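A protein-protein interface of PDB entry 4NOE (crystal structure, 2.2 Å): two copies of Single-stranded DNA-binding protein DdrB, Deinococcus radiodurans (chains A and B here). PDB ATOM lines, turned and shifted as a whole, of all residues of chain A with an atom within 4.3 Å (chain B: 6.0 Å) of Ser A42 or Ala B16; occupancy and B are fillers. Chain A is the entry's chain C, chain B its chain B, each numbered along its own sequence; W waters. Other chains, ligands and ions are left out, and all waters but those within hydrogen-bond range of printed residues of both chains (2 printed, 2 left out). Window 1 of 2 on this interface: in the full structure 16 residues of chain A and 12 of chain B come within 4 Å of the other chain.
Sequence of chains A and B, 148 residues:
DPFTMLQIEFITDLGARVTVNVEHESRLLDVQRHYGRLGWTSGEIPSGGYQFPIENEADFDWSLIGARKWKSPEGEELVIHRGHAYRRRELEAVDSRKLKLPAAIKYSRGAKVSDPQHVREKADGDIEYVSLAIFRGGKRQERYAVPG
Position printed for both chains: 10.
Water W2 lies within hydrogen-bond range of the side-chain amide nitrogen of Gln A32 (2.5 Å) and the side-chain hydroxyl of Thr B12 (2.7 Å). Water W1 lies within hydrogen-bond range of O of Leu B14 (2.7 Å), O of Ser A42 (2.8 Å) and N of Ala B16 (3.4 Å).
Ser A42 touches three residues of chain B. Ala B16 touches just these residues of chain A: Gln A32 and Ser A42. Of the printed residues of chain B, Gly A43 touches Gly B15 and Arg B17. Printed residues of chain A within 4 Å of Leu B14: Gln A32 (3.9 Å). Of the printed residues of chain B, Gln A32 touches Leu B14 (3.9 Å) and Ala B16 (3.8 Å). Printed residues of chain A within 4 Å of Arg B17: Ile A8, Glu A9, Ser A42 and Gly A43. Val B18 touches none of the printed residues of chain A. Thr A41 touches none of the printed residues of chain B.
Arg B17 touches Ile A8 (O to CA, 3.3 Å). Gln A32 touches Leu B14 (OE1 to CD1, 3.9 Å). Ala B16 touches Gln A32. Ala B16 touches Ser A42 (CA to OG, 3.4 Å). Gly A43 touches Gly B15. CG of Arg B17 touches N of Gly A43 (3.4 Å).
Hydrophobic or aromatic side chains of chain A that line the printed part of chain B: Ile A8. Among the printed residues, no Asp or Glu carboxylate lies within 4 Å of a Lys or Arg side-chain nitrogen of the other chain.
The backbone NH of Ala B16 is in hydrogen-bond range of the side-chain hydroxyl of Thr B12, at 3.1 Å. The backbone NH (N) of Leu B14 lies close to the side-chain hydroxyl (OG1) of Thr B12 (3.1 Å). O of Glu A9 sits at hydrogen-bond distance from OG of Ser A42. OG1 of Thr B12 sits at hydrogen-bond distance from N of Gly B15, 3.5 Å away.
O of Ser A42 sits close to O of Gly B15 (3.4 Å). O of Arg B17 sits at hydrogen-bond distance from N of Glu A9, 3.0 Å away. The backbone NH (N) of Arg B17 lies within hydrogen-bond range of the side-chain hydroxyl (OG) of Ser A42 (2.9 Å).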
ATOM      1  N   ILE A   8      27.105 -19.838  -4.315  1.00  0.00           N
ATOM      2  CA  ILE A   8      25.770 -19.947  -3.772  1.00  0.00           C
ATOM      3  C   ILE A   8      25.084 -21.126  -4.453  1.00  0.00           C
ATOM      4  O   ILE A   8      25.240 -21.338  -5.660  1.00  0.00           O
ATOM      5  CB  ILE A   8      24.990 -18.604  -3.896  1.00  0.00           C
ATOM      6  CG1 ILE A   8      23.543 -18.752  -3.409  1.00  0.00           C
ATOM      7  CG2 ILE A   8      25.039 -18.067  -5.317  1.00  0.00           C
ATOM      8  CD1 ILE A   8      22.754 -17.425  -3.407  1.00  0.00           C
ATOM      9  N   GLU A   9      24.367 -21.917  -3.665  1.00  0.00           N
ATOM     10  CA  GLU A   9      23.662 -23.072  -4.187  1.00  0.00           C
ATOM     11  C   GLU A   9      22.185 -22.748  -4.344  1.00  0.00           C
ATOM     12  O   GLU A   9      21.563 -22.262  -3.406  1.00  0.00           O
ATOM     13  CB  GLU A   9      23.834 -24.257  -3.237  1.00  0.00           C
ATOM     14  N   PHE A  10      21.635 -23.009  -5.531  1.00  0.00           N
ATOM     15  CA  PHE A  10      20.230 -22.727  -5.822  1.00  0.00           C
ATOM     16  C   PHE A  10      19.432 -23.995  -6.103  1.00  0.00           C
ATOM     17  O   PHE A  10      19.989 -25.027  -6.502  1.00  0.00           O
ATOM     18  CB  PHE A  10      20.078 -21.811  -7.055  1.00  0.00           C
ATOM     19  CG  PHE A  10      20.442 -20.353  -6.813  1.00  0.00           C
ATOM     20  CD1 PHE A  10      19.566 -19.499  -6.141  1.00  0.00           C
ATOM     21  CD2 PHE A  10      21.632 -19.829  -7.301  1.00  0.00           C
ATOM     22  CE1 PHE A  10      19.883 -18.169  -5.920  1.00  0.00           C
ATOM     23  CE2 PHE A  10      21.964 -18.473  -7.095  1.00  0.00           C
ATOM     24  CZ  PHE A  10      21.085 -17.650  -6.410  1.00  0.00           C
ATOM     25  N   GLN A  32      21.627 -12.969  -5.993  1.00  0.00           N
ATOM     26  CA  GLN A  32      20.402 -13.513  -5.452  1.00  0.00           C
ATOM     27  C   GLN A  32      19.184 -12.975  -6.192  1.00  0.00           C
ATOM     28  O   GLN A  32      18.286 -13.745  -6.524  1.00  0.00           O
ATOM     29  CB  GLN A  32      20.298 -13.252  -3.950  1.00  0.00           C
ATOM     30  CG  GLN A  32      20.708 -14.444  -3.098  1.00  0.00           C
ATOM     31  CD  GLN A  32      20.514 -14.193  -1.616  1.00  0.00           C
ATOM     32  OE1 GLN A  32      19.409 -14.336  -1.085  1.00  0.00           O
ATOM     33  NE2 GLN A  32      21.584 -13.808  -0.944  1.00  0.00           N
ATOM     34  N   THR A  41      15.526 -20.458  -5.875  1.00  0.00           N
ATOM     35  CA  THR A  41      15.607 -20.162  -4.460  1.00  0.00           C
ATOM     36  C   THR A  41      16.880 -20.761  -3.903  1.00  0.00           C
ATOM     37  O   THR A  41      17.431 -21.692  -4.473  1.00  0.00           O
ATOM     38  CB  THR A  41      14.418 -20.737  -3.691  1.00  0.00           C
ATOM     39  OG1 THR A  41      14.380 -22.159  -3.871  1.00  0.00           O
ATOM     40  CG2 THR A  41      13.117 -20.122  -4.178  1.00  0.00           C
ATOM     41  N   SER A  42      17.339 -20.218  -2.785  1.00  0.00           N
ATOM     42  CA  SER A  42      18.549 -20.691  -2.144  1.00  0.00           C
ATOM     43  C   SER A  42      18.215 -20.959  -0.692  1.00  0.00           C
ATOM     44  O   SER A  42      17.719 -20.074   0.017  1.00  0.00           O
ATOM     45  CB  SER A  42      19.646 -19.637  -2.248  1.00  0.00           C
ATOM     46  OG  SER A  42      20.855 -20.123  -1.697  1.00  0.00           O
ATOM     47  N   GLY A  43      18.467 -22.184  -0.246  1.00  0.00           N
ATOM     48  CA  GLY A  43      18.107 -22.564   1.104  1.00  0.00           C
ATOM     49  C   GLY A  43      16.639 -22.914   1.235  1.00  0.00           C
ATOM     50  O   GLY A  43      15.899 -22.970   0.250  1.00  0.00           O
ATOM     51  N   GLU A  44      16.217 -23.135   2.472  1.00  0.00           N
ATOM     52  CA  GLU A  44      14.857 -23.542   2.766  1.00  0.00           C
ATOM     53  C   GLU A  44      14.120 -22.385   3.421  1.00  0.00           C
ATOM     54  O   GLU A  44      14.748 -21.514   4.015  1.00  0.00           O
ATOM     55  CB  GLU A  44      14.887 -24.746   3.735  1.00  0.00           C
ATOM     56  N   PHE B  10      27.851 -21.531   4.754  1.00  0.00           N
ATOM     57  CA  PHE B  10      27.015 -20.732   5.639  1.00  0.00           C
ATOM     58  C   PHE B  10      25.563 -20.753   5.167  1.00  0.00           C
ATOM     59  O   PHE B  10      25.295 -20.933   3.973  1.00  0.00           O
ATOM     60  CB  PHE B  10      27.485 -19.263   5.638  1.00  0.00           C
ATOM     61  CG  PHE B  10      28.767 -19.019   6.408  1.00  0.00           C
ATOM     62  CD1 PHE B  10      28.778 -19.057   7.799  1.00  0.00           C
ATOM     63  CD2 PHE B  10      29.956 -18.741   5.739  1.00  0.00           C
ATOM     64  CE1 PHE B  10      29.962 -18.843   8.514  1.00  0.00           C
ATOM     65  CE2 PHE B  10      31.147 -18.517   6.448  1.00  0.00           C
ATOM     66  CZ  PHE B  10      31.145 -18.570   7.838  1.00  0.00           C
ATOM     67  N   ILE B  11      24.638 -20.569   6.109  1.00  0.00           N
ATOM     68  CA  ILE B  11      23.292 -20.122   5.787  1.00  0.00           C
ATOM     69  C   ILE B  11      23.239 -18.625   6.128  1.00  0.00           C
ATOM     70  O   ILE B  11      23.478 -18.238   7.279  1.00  0.00           O
ATOM     71  CB  ILE B  11      22.229 -20.888   6.607  1.00  0.00           C
ATOM     72  CG1 ILE B  11      22.306 -22.390   6.306  1.00  0.00           C
ATOM     73  CG2 ILE B  11      20.842 -20.345   6.312  1.00  0.00           C
ATOM     74  CD1 ILE B  11      22.076 -22.740   4.841  1.00  0.00           C
ATOM     75  N   THR B  12      22.937 -17.780   5.142  1.00  0.00           N
ATOM     76  CA  THR B  12      23.012 -16.334   5.337  1.00  0.00           C
ATOM     77  C   THR B  12      21.809 -15.799   6.109  1.00  0.00           C
ATOM     78  O   THR B  12      20.914 -16.556   6.489  1.00  0.00           O
ATOM     79  CB  THR B  12      23.113 -15.591   3.987  1.00  0.00           C
ATOM     80  OG1 THR B  12      21.842 -15.616   3.319  1.00  0.00           O
ATOM     81  CG2 THR B  12      24.135 -16.269   3.103  1.00  0.00           C
ATOM     82  N   ASP B  13      21.793 -14.492   6.339  1.00  0.00           N
ATOM     83  CA  ASP B  13      20.652 -13.857   6.995  1.00  0.00           C
ATOM     84  C   ASP B  13      19.382 -14.006   6.149  1.00  0.00           C
ATOM     85  O   ASP B  13      18.279 -13.888   6.668  1.00  0.00           O
ATOM     86  CB  ASP B  13      20.941 -12.375   7.311  1.00  0.00           C
ATOM     87  CG  ASP B  13      21.466 -11.600   6.109  1.00  0.00           C
ATOM     88  OD1 ASP B  13      22.405 -12.089   5.427  1.00  0.00           O
ATOM     89  OD2 ASP B  13      20.952 -10.481   5.852  1.00  0.00           O
ATOM     90  N   LEU B  14      19.538 -14.274   4.852  1.00  0.00           N
ATOM     91  CA  LEU B  14      18.374 -14.464   3.979  1.00  0.00           C
ATOM     92  C   LEU B  14      18.128 -15.954   3.722  1.00  0.00           C
ATOM     93  O   LEU B  14      17.336 -16.330   2.852  1.00  0.00           O
ATOM     94  CB  LEU B  14      18.556 -13.697   2.654  1.00  0.00           C
ATOM     95  CG  LEU B  14      18.312 -12.183   2.735  1.00  0.00           C
ATOM     96  CD1 LEU B  14      18.773 -11.474   1.467  1.00  0.00           C
ATOM     97  CD2 LEU B  14      16.833 -11.900   3.003  1.00  0.00           C
ATOM     98  N   GLY B  15      18.815 -16.806   4.479  1.00  0.00           N
ATOM     99  CA  GLY B  15      18.633 -18.248   4.344  1.00  0.00           C
ATOM    100  C   GLY B  15      19.405 -18.857   3.183  1.00  0.00           C
ATOM    101  O   GLY B  15      19.379 -20.069   2.984  1.00  0.00           O
ATOM    102  N   ALA B  16      20.102 -18.028   2.412  1.00  0.00           N
ATOM    103  CA  ALA B  16      20.845 -18.530   1.253  1.00  0.00           C
ATOM    104  C   ALA B  16      22.004 -19.454   1.657  1.00  0.00           C
ATOM    105  O   ALA B  16      22.673 -19.220   2.675  1.00  0.00           O
ATOM    106  CB  ALA B  16      21.360 -17.359   0.427  1.00  0.00           C
ATOM    107  N   ARG B  17      22.264 -20.489   0.861  1.00  0.00           N
ATOM    108  CA  ARG B  17      23.399 -21.385   1.139  1.00  0.00           C
ATOM    109  C   ARG B  17      24.634 -20.943   0.380  1.00  0.00           C
ATOM    110  O   ARG B  17      24.725 -21.135  -0.843  1.00  0.00           O
ATOM    111  CB  ARG B  17      23.094 -22.858   0.794  1.00  0.00           C
ATOM    112  CG  ARG B  17      21.658 -23.166   0.545  1.00  0.00           C
ATOM    113  CD  ARG B  17      21.167 -24.311   1.427  1.00  0.00           C
ATOM    114  NE  ARG B  17      22.196 -25.303   1.725  1.00  0.00           N
ATOM    115  CZ  ARG B  17      22.626 -26.218   0.863  1.00  0.00           C
ATOM    116  NH1 ARG B  17      22.134 -26.261  -0.370  1.00  0.00           N
ATOM    117  NH2 ARG B  17      23.559 -27.085   1.232  1.00  0.00           N
ATOM    118  N   VAL B  18      25.576 -20.354   1.110  1.00  0.00           N
ATOM    119  CA  VAL B  18      26.745 -19.737   0.510  1.00  0.00           C
ATOM    120  C   VAL B  18      28.007 -20.390   1.048  1.00  0.00           C
ATOM    121  O   VAL B  18      28.097 -20.714   2.244  1.00  0.00           O
ATOM    122  CB  VAL B  18      26.756 -18.208   0.763  1.00  0.00           C
ATOM    123  CG1 VAL B  18      28.048 -17.581   0.261  1.00  0.00           C
ATOM    124  CG2 VAL B  18      25.583 -17.573   0.067  1.00  0.00           C
HETATM  125  O   HOH W   1      17.435 -17.339   0.359  1.00  0.00           O
HETATM  126  O   HOH W   2      22.121 -13.703   1.455  1.00  0.00           O
